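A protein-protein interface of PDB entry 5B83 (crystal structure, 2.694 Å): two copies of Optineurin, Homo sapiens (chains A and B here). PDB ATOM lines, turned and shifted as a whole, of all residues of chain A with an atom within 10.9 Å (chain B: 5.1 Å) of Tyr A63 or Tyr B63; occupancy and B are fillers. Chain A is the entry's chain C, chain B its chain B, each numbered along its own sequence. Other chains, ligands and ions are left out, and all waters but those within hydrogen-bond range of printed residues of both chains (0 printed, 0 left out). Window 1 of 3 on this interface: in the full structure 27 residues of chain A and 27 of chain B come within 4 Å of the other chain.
Gln A59 touches Met B60, and with the chains exchanged Met A60 touches Gln B59.
Met A60 touches Tyr B63, and with the chains exchanged Tyr A63 touches Met B60.
Tyr A63 touches Cys B64, but with the chains exchanged Cys A64 does not touch Tyr B63 (4.3 Å).
Phe A67 touches its own counterpart, Phe B67.
SD of Met B60 sits at hydrogen-bond distance from NE2 of Gln A59, 3.6 Å away.
Printed residues of chain A that touch a printed residue of chain B: Gln A59, Met A60, Tyr A63, Asp A66, Phe A67 and Glu A70.
Hydrophobic or aromatic side chains of chain A that line the printed part of chain B: Met A60, Tyr A63 and Phe A67.
Along chain A the printed residues that touch a printed residue of chain B span positions 59 to 70.
Of the 9 printed residues of chain B, 6 touch a printed residue of chain A.
Hydrophobic or aromatic side chains of chain B that line the printed part of chain A: Met B60, Tyr B63 and Phe B67.
Among the printed residues, no Asp or Glu carboxylate lies within 4 Å of a Lys or Arg side-chain nitrogen of the other chain.
Tyr A63 touches just these residues of chain B: Met B60 (3.6 Å), Tyr B63 (3.96 Å) and Cys B64 (3.6 Å).
Tyr B63 touches just these residues of chain A: Met A60 (3.6 Å) and Tyr A63 (3.96 Å).
No residue of chain A comes within 4 Å of Val B62.
Cys B64 touches just one residue of chain A: Tyr A63.
No residue of chain A comes within 4 Å of Ser B65.
Asp B66 touches just one residue of chain A: Phe A67.
Of the printed residues of chain B, Met A60 touches Gln B59 (3.7 Å) and Tyr B63 (3.6 Å).
Printed residues of chain B within 4 Å of Glu A70: Phe B67.
Met A60 touches Gln B59 (CE to CG, 3.7 Å).
Tyr B63 touches Met A60.
Met B60 touches Tyr A63 (O to CD2, 3.6 Å).
Tyr B63 touches Tyr A63 (CB to CB, 3.96 Å).
Tyr A63 touches Cys B64 (CE2 to CB, 3.6 Å).
Asp A66 touches Phe B67.
O of Asp B66 touches CD1 of Phe A67, at 3.97 Å.
N of Phe B67 touches CD1 of Phe A67, 3.96 Å away.
Glu A70 touches Phe B67 (CG to CE1, 3.4 Å).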
ATOM      1  N   ILE A  55     -37.061  27.634  26.186  1.00  0.00           N
ATOM      2  CA  ILE A  55     -35.658  27.401  26.522  1.00  0.00           C
ATOM      3  C   ILE A  55     -35.288  25.941  26.317  1.00  0.00           C
ATOM      4  O   ILE A  55     -34.147  25.623  25.961  1.00  0.00           O
ATOM      5  CB  ILE A  55     -35.362  27.832  27.967  1.00  0.00           C
ATOM      6  CG1 ILE A  55     -36.055  29.163  28.278  1.00  0.00           C
ATOM      7  CG2 ILE A  55     -33.871  27.908  28.189  1.00  0.00           C
ATOM      8  CD1 ILE A  55     -35.735  30.270  27.286  1.00  0.00           C
ATOM      9  N   LEU A  56     -36.225  25.026  26.581  1.00  0.00           N
ATOM     10  CA  LEU A  56     -35.966  23.622  26.305  1.00  0.00           C
ATOM     11  C   LEU A  56     -35.909  23.384  24.808  1.00  0.00           C
ATOM     12  O   LEU A  56     -34.996  22.706  24.315  1.00  0.00           O
ATOM     13  CB  LEU A  56     -37.040  22.736  26.937  1.00  0.00           C
ATOM     14  CG  LEU A  56     -37.278  22.764  28.447  1.00  0.00           C
ATOM     15  CD1 LEU A  56     -38.359  21.779  28.818  1.00  0.00           C
ATOM     16  CD2 LEU A  56     -36.032  22.425  29.180  1.00  0.00           C
ATOM     17  N   ARG A  57     -36.869  23.947  24.067  1.00  0.00           N
ATOM     18  CA  ARG A  57     -36.899  23.729  22.625  1.00  0.00           C
ATOM     19  C   ARG A  57     -35.616  24.234  21.977  1.00  0.00           C
ATOM     20  O   ARG A  57     -35.031  23.547  21.134  1.00  0.00           O
ATOM     21  CB  ARG A  57     -38.130  24.396  22.018  1.00  0.00           C
ATOM     22  CG  ARG A  57     -38.906  23.507  21.046  1.00  0.00           C
ATOM     23  CD  ARG A  57     -40.392  23.912  20.986  1.00  0.00           C
ATOM     24  NE  ARG A  57     -41.252  22.728  20.965  1.00  0.00           N
ATOM     25  CZ  ARG A  57     -42.510  22.679  21.420  1.00  0.00           C
ATOM     26  NH1 ARG A  57     -43.089  23.760  21.945  1.00  0.00           N
ATOM     27  NH2 ARG A  57     -43.193  21.536  21.358  1.00  0.00           N
ATOM     28  N   ALA A  58     -35.147  25.417  22.387  1.00  0.00           N
ATOM     29  CA  ALA A  58     -33.875  25.925  21.893  1.00  0.00           C
ATOM     30  C   ALA A  58     -32.718  25.022  22.312  1.00  0.00           C
ATOM     31  O   ALA A  58     -31.797  24.764  21.520  1.00  0.00           O
ATOM     32  CB  ALA A  58     -33.652  27.349  22.399  1.00  0.00           C
ATOM     33  N   GLN A  59     -32.743  24.526  23.549  1.00  0.00           N
ATOM     34  CA  GLN A  59     -31.676  23.630  23.958  1.00  0.00           C
ATOM     35  C   GLN A  59     -31.757  22.299  23.223  1.00  0.00           C
ATOM     36  O   GLN A  59     -30.722  21.700  22.916  1.00  0.00           O
ATOM     37  CB  GLN A  59     -31.707  23.421  25.468  1.00  0.00           C
ATOM     38  CG  GLN A  59     -30.655  22.431  25.932  1.00  0.00           C
ATOM     39  CD  GLN A  59     -29.817  22.954  27.070  1.00  0.00           C
ATOM     40  OE1 GLN A  59     -28.760  23.563  26.862  1.00  0.00           O
ATOM     41  NE2 GLN A  59     -30.281  22.717  28.293  1.00  0.00           N
ATOM     42  N   MET A  60     -32.966  21.833  22.918  1.00  0.00           N
ATOM     43  CA  MET A  60     -33.111  20.637  22.087  1.00  0.00           C
ATOM     44  C   MET A  60     -32.427  20.821  20.745  1.00  0.00           C
ATOM     45  O   MET A  60     -31.632  19.973  20.321  1.00  0.00           O
ATOM     46  CB  MET A  60     -34.588  20.326  21.861  1.00  0.00           C
ATOM     47  CG  MET A  60     -35.163  19.244  22.697  1.00  0.00           C
ATOM     48  SD  MET A  60     -36.896  19.131  22.253  1.00  0.00           S
ATOM     49  CE  MET A  60     -36.810  18.437  20.600  1.00  0.00           C
ATOM     50  N   GLU A  61     -32.745  21.926  20.054  1.00  0.00           N
ATOM     51  CA  GLU A  61     -32.144  22.206  18.757  1.00  0.00           C
ATOM     52  C   GLU A  61     -30.624  22.151  18.831  1.00  0.00           C
ATOM     53  O   GLU A  61     -29.976  21.558  17.960  1.00  0.00           O
ATOM     54  CB  GLU A  61     -32.632  23.558  18.235  1.00  0.00           C
ATOM     55  CG  GLU A  61     -34.132  23.562  17.905  1.00  0.00           C
ATOM     56  CD  GLU A  61     -34.820  24.927  18.123  1.00  0.00           C
ATOM     57  OE1 GLU A  61     -34.126  25.978  18.090  1.00  0.00           O
ATOM     58  OE2 GLU A  61     -36.062  24.941  18.328  1.00  0.00           O
ATOM     59  N   VAL A  62     -30.039  22.716  19.889  1.00  0.00           N
ATOM     60  CA  VAL A  62     -28.586  22.785  19.984  1.00  0.00           C
ATOM     61  C   VAL A  62     -27.991  21.398  20.205  1.00  0.00           C
ATOM     62  O   VAL A  62     -27.047  20.992  19.512  1.00  0.00           O
ATOM     63  CB  VAL A  62     -28.173  23.764  21.092  1.00  0.00           C
ATOM     64  CG1 VAL A  62     -26.713  23.560  21.448  1.00  0.00           C
ATOM     65  CG2 VAL A  62     -28.419  25.197  20.632  1.00  0.00           C
ATOM     66  N   TYR A  63     -28.520  20.653  21.180  1.00  0.00           N
ATOM     67  CA  TYR A  63     -28.040  19.288  21.358  1.00  0.00           C
ATOM     68  C   TYR A  63     -28.178  18.491  20.073  1.00  0.00           C
ATOM     69  O   TYR A  63     -27.362  17.617  19.780  1.00  0.00           O
ATOM     70  CB  TYR A  63     -28.812  18.566  22.453  1.00  0.00           C
ATOM     71  CG  TYR A  63     -28.558  19.022  23.859  1.00  0.00           C
ATOM     72  CD1 TYR A  63     -27.706  20.073  24.147  1.00  0.00           C
ATOM     73  CD2 TYR A  63     -29.178  18.383  24.910  1.00  0.00           C
ATOM     74  CE1 TYR A  63     -27.492  20.468  25.466  1.00  0.00           C
ATOM     75  CE2 TYR A  63     -28.966  18.758  26.209  1.00  0.00           C
ATOM     76  CZ  TYR A  63     -28.129  19.797  26.492  1.00  0.00           C
ATOM     77  OH  TYR A  63     -27.959  20.133  27.815  1.00  0.00           O
ATOM     78  N   CYS A  64     -29.198  18.783  19.289  1.00  0.00           N
ATOM     79  CA  CYS A  64     -29.366  18.073  18.037  1.00  0.00           C
ATOM     80  C   CYS A  64     -28.188  18.324  17.106  1.00  0.00           C
ATOM     81  O   CYS A  64     -27.515  17.386  16.674  1.00  0.00           O
ATOM     82  CB  CYS A  64     -30.679  18.503  17.397  1.00  0.00           C
ATOM     83  SG  CYS A  64     -31.508  17.187  16.605  1.00  0.00           S
ATOM     84  N   SER A  65     -27.919  19.593  16.788  1.00  0.00           N
ATOM     85  CA  SER A  65     -26.845  19.868  15.844  1.00  0.00           C
ATOM     86  C   SER A  65     -25.481  19.524  16.431  1.00  0.00           C
ATOM     87  O   SER A  65     -24.553  19.214  15.677  1.00  0.00           O
ATOM     88  CB  SER A  65     -26.894  21.323  15.379  1.00  0.00           C
ATOM     89  OG  SER A  65     -26.786  22.189  16.481  1.00  0.00           O
ATOM     90  N   ASP A  66     -25.344  19.555  17.761  1.00  0.00           N
ATOM     91  CA  ASP A  66     -24.123  19.052  18.384  1.00  0.00           C
ATOM     92  C   ASP A  66     -23.910  17.577  18.062  1.00  0.00           C
ATOM     93  O   ASP A  66     -22.797  17.151  17.723  1.00  0.00           O
ATOM     94  CB  ASP A  66     -24.171  19.253  19.896  1.00  0.00           C
ATOM     95  CG  ASP A  66     -23.884  20.677  20.307  1.00  0.00           C
ATOM     96  OD1 ASP A  66     -23.454  21.492  19.462  1.00  0.00           O
ATOM     97  OD2 ASP A  66     -24.093  20.984  21.495  1.00  0.00           O
ATOM     98  N   PHE A  67     -24.976  16.789  18.158  1.00  0.00           N
ATOM     99  CA  PHE A  67     -24.920  15.384  17.790  1.00  0.00           C
ATOM    100  C   PHE A  67     -24.518  15.195  16.326  1.00  0.00           C
ATOM    101  O   PHE A  67     -23.695  14.332  16.009  1.00  0.00           O
ATOM    102  CB  PHE A  67     -26.280  14.723  18.069  1.00  0.00           C
ATOM    103  CG  PHE A  67     -26.368  13.358  17.525  1.00  0.00           C
ATOM    104  CD1 PHE A  67     -25.826  12.296  18.224  1.00  0.00           C
ATOM    105  CD2 PHE A  67     -26.902  13.139  16.270  1.00  0.00           C
ATOM    106  CE1 PHE A  67     -25.850  11.018  17.694  1.00  0.00           C
ATOM    107  CE2 PHE A  67     -26.939  11.863  15.727  1.00  0.00           C
ATOM    108  CZ  PHE A  67     -26.421  10.803  16.437  1.00  0.00           C
ATOM    109  N   HIS A  68     -25.087  15.987  15.419  1.00  0.00           N
ATOM    110  CA  HIS A  68     -24.718  15.847  14.019  1.00  0.00           C
ATOM    111  C   HIS A  68     -23.281  16.242  13.758  1.00  0.00           C
ATOM    112  O   HIS A  68     -22.645  15.667  12.867  1.00  0.00           O
ATOM    113  CB  HIS A  68     -25.680  16.634  13.148  1.00  0.00           C
ATOM    114  CG  HIS A  68     -27.006  15.954  13.062  1.00  0.00           C
ATOM    115  ND1 HIS A  68     -28.178  16.524  13.512  1.00  0.00           N
ATOM    116  CD2 HIS A  68     -27.316  14.685  12.707  1.00  0.00           C
ATOM    117  CE1 HIS A  68     -29.162  15.658  13.379  1.00  0.00           C
ATOM    118  NE2 HIS A  68     -28.664  14.533  12.899  1.00  0.00           N
ATOM    119  N   ALA A  69     -22.756  17.203  14.525  1.00  0.00           N
ATOM    120  CA  ALA A  69     -21.360  17.568  14.397  1.00  0.00           C
ATOM    121  C   ALA A  69     -20.459  16.408  14.803  1.00  0.00           C
ATOM    122  O   ALA A  69     -19.488  16.101  14.105  1.00  0.00           O
ATOM    123  CB  ALA A  69     -21.083  18.804  15.235  1.00  0.00           C
ATOM    124  N   GLU A  70     -20.785  15.716  15.897  1.00  0.00           N
ATOM    125  CA  GLU A  70     -19.951  14.592  16.287  1.00  0.00           C
ATOM    126  C   GLU A  70     -19.982  13.499  15.236  1.00  0.00           C
ATOM    127  O   GLU A  70     -18.942  12.953  14.867  1.00  0.00           O
ATOM    128  CB  GLU A  70     -20.375  14.024  17.644  1.00  0.00           C
ATOM    129  CG  GLU A  70     -19.912  14.809  18.867  1.00  0.00           C
ATOM    130  CD  GLU A  70     -18.396  14.966  18.960  1.00  0.00           C
ATOM    131  OE1 GLU A  70     -17.689  13.941  18.876  1.00  0.00           O
ATOM    132  OE2 GLU A  70     -17.922  16.122  19.108  1.00  0.00           O
ATOM    133  N   ARG A  71     -21.171  13.142  14.759  1.00  0.00           N
ATOM    134  CA  ARG A  71     -21.248  12.062  13.778  1.00  0.00           C
ATOM    135  C   ARG A  71     -20.524  12.441  12.488  1.00  0.00           C
ATOM    136  O   ARG A  71     -19.856  11.601  11.878  1.00  0.00           O
ATOM    137  CB  ARG A  71     -22.707  11.680  13.507  1.00  0.00           C
ATOM    138  CG  ARG A  71     -22.856  10.869  12.273  1.00  0.00           C
ATOM    139  CD  ARG A  71     -24.087  10.033  12.299  1.00  0.00           C
ATOM    140  NE  ARG A  71     -24.033   9.165  13.457  1.00  0.00           N
ATOM    141  CZ  ARG A  71     -24.921   8.228  13.725  1.00  0.00           C
ATOM    142  NH1 ARG A  71     -25.957   8.041  12.921  1.00  0.00           N
ATOM    143  NH2 ARG A  71     -24.761   7.481  14.796  1.00  0.00           N
ATOM    144  N   GLN B  59     -37.070  14.478  26.269  1.00  0.00           N
ATOM    145  CA  GLN B  59     -36.560  14.417  24.905  1.00  0.00           C
ATOM    146  C   GLN B  59     -35.219  15.126  24.788  1.00  0.00           C
ATOM    147  O   GLN B  59     -34.355  14.704  24.016  1.00  0.00           O
ATOM    148  CB  GLN B  59     -37.579  15.044  23.966  1.00  0.00           C
ATOM    149  CG  GLN B  59     -37.083  15.299  22.572  1.00  0.00           C
ATOM    150  CD  GLN B  59     -37.304  14.136  21.657  1.00  0.00           C
ATOM    151  OE1 GLN B  59     -36.519  13.202  21.647  1.00  0.00           O
ATOM    152  NE2 GLN B  59     -38.386  14.179  20.878  1.00  0.00           N
ATOM    153  N   MET B  60     -35.031  16.193  25.561  1.00  0.00           N
ATOM    154  CA  MET B  60     -33.745  16.866  25.636  1.00  0.00           C
ATOM    155  C   MET B  60     -32.698  15.980  26.306  1.00  0.00           C
ATOM    156  O   MET B  60     -31.571  15.855  25.811  1.00  0.00           O
ATOM    157  CB  MET B  60     -33.922  18.182  26.386  1.00  0.00           C
ATOM    158  CG  MET B  60     -32.794  19.179  26.297  1.00  0.00           C
ATOM    159  SD  MET B  60     -32.784  20.179  27.799  1.00  0.00           S
ATOM    160  CE  MET B  60     -32.158  18.973  28.974  1.00  0.00           C
ATOM    161  N   GLU B  61     -33.046  15.339  27.426  1.00  0.00           N
ATOM    162  CA  GLU B  61     -32.065  14.458  28.068  1.00  0.00           C
ATOM    163  C   GLU B  61     -31.606  13.371  27.101  1.00  0.00           C
ATOM    164  O   GLU B  61     -30.417  13.038  27.035  1.00  0.00           O
ATOM    165  CB  GLU B  61     -32.634  13.832  29.354  1.00  0.00           C
ATOM    166  CG  GLU B  61     -33.080  14.820  30.441  1.00  0.00           C
ATOM    167  CD  GLU B  61     -33.810  14.156  31.639  1.00  0.00           C
ATOM    168  OE1 GLU B  61     -33.571  12.961  31.935  1.00  0.00           O
ATOM    169  OE2 GLU B  61     -34.626  14.841  32.300  1.00  0.00           O
ATOM    170  N   VAL B  62     -32.535  12.829  26.321  1.00  0.00           N
ATOM    171  CA  VAL B  62     -32.205  11.750  25.404  1.00  0.00           C
ATOM    172  C   VAL B  62     -31.262  12.253  24.314  1.00  0.00           C
ATOM    173  O   VAL B  62     -30.273  11.594  23.968  1.00  0.00           O
ATOM    174  CB  VAL B  62     -33.518  11.146  24.849  1.00  0.00           C
ATOM    175  CG1 VAL B  62     -33.309  10.424  23.552  1.00  0.00           C
ATOM    176  CG2 VAL B  62     -34.142  10.185  25.882  1.00  0.00           C
ATOM    177  N   TYR B  63     -31.531  13.442  23.773  1.00  0.00           N
ATOM    178  CA  TYR B  63     -30.581  14.025  22.841  1.00  0.00           C
ATOM    179  C   TYR B  63     -29.234  14.246  23.507  1.00  0.00           C
ATOM    180  O   TYR B  63     -28.201  14.197  22.834  1.00  0.00           O
ATOM    181  CB  TYR B  63     -31.098  15.342  22.265  1.00  0.00           C
ATOM    182  CG  TYR B  63     -32.239  15.232  21.272  1.00  0.00           C
ATOM    183  CD1 TYR B  63     -32.636  14.003  20.747  1.00  0.00           C
ATOM    184  CD2 TYR B  63     -32.926  16.365  20.858  1.00  0.00           C
ATOM    185  CE1 TYR B  63     -33.682  13.920  19.829  1.00  0.00           C
ATOM    186  CE2 TYR B  63     -33.979  16.281  19.967  1.00  0.00           C
ATOM    187  CZ  TYR B  63     -34.353  15.060  19.454  1.00  0.00           C
ATOM    188  OH  TYR B  63     -35.393  14.995  18.570  1.00  0.00           O
ATOM    189  N   CYS B  64     -29.208  14.460  24.824  1.00  0.00           N
ATOM    190  CA  CYS B  64     -27.926  14.671  25.478  1.00  0.00           C
ATOM    191  C   CYS B  64     -27.145  13.370  25.593  1.00  0.00           C
ATOM    192  O   CYS B  64     -25.980  13.305  25.195  1.00  0.00           O
ATOM    193  CB  CYS B  64     -28.112  15.320  26.844  1.00  0.00           C
ATOM    194  SG  CYS B  64     -26.535  15.549  27.738  1.00  0.00           S
ATOM    195  N   SER B  65     -27.761  12.314  26.124  1.00  0.00           N
ATOM    196  CA  SER B  65     -27.039  11.047  26.205  1.00  0.00           C
ATOM    197  C   SER B  65     -26.610  10.523  24.830  1.00  0.00           C
ATOM    198  O   SER B  65     -25.583   9.836  24.734  1.00  0.00           O
ATOM    199  CB  SER B  65     -27.886  10.003  26.933  1.00  0.00           C
ATOM    200  OG  SER B  65     -29.206  10.026  26.466  1.00  0.00           O
ATOM    201  N   ASP B  66     -27.351  10.846  23.763  1.00  0.00           N
ATOM    202  CA  ASP B  66     -26.966  10.369  22.440  1.00  0.00           C
ATOM    203  C   ASP B  66     -25.659  11.000  22.003  1.00  0.00           C
ATOM    204  O   ASP B  66     -24.763  10.317  21.501  1.00  0.00           O
ATOM    205  CB  ASP B  66     -28.066  10.665  21.424  1.00  0.00           C
ATOM    206  CG  ASP B  66     -29.256   9.734  21.565  1.00  0.00           C
ATOM    207  OD1 ASP B  66     -29.094   8.627  22.139  1.00  0.00           O
ATOM    208  OD2 ASP B  66     -30.353  10.110  21.082  1.00  0.00           O
ATOM    209  N   PHE B  67     -25.543  12.316  22.175  1.00  0.00           N
ATOM    210  CA  PHE B  67     -24.298  13.003  21.888  1.00  0.00           C
ATOM    211  C   PHE B  67     -23.126  12.307  22.565  1.00  0.00           C
ATOM    212  O   PHE B  67     -22.116  12.000  21.932  1.00  0.00           O
ATOM    213  CB  PHE B  67     -24.413  14.463  22.321  1.00  0.00           C
ATOM    214  CG  PHE B  67     -23.104  15.135  22.496  1.00  0.00           C
ATOM    215  CD1 PHE B  67     -22.469  15.719  21.420  1.00  0.00           C
ATOM    216  CD2 PHE B  67     -22.495  15.171  23.743  1.00  0.00           C
ATOM    217  CE1 PHE B  67     -21.238  16.335  21.582  1.00  0.00           C
ATOM    218  CE2 PHE B  67     -21.271  15.768  23.906  1.00  0.00           C
ATOM    219  CZ  PHE B  67     -20.634  16.351  22.822  1.00  0.00           C
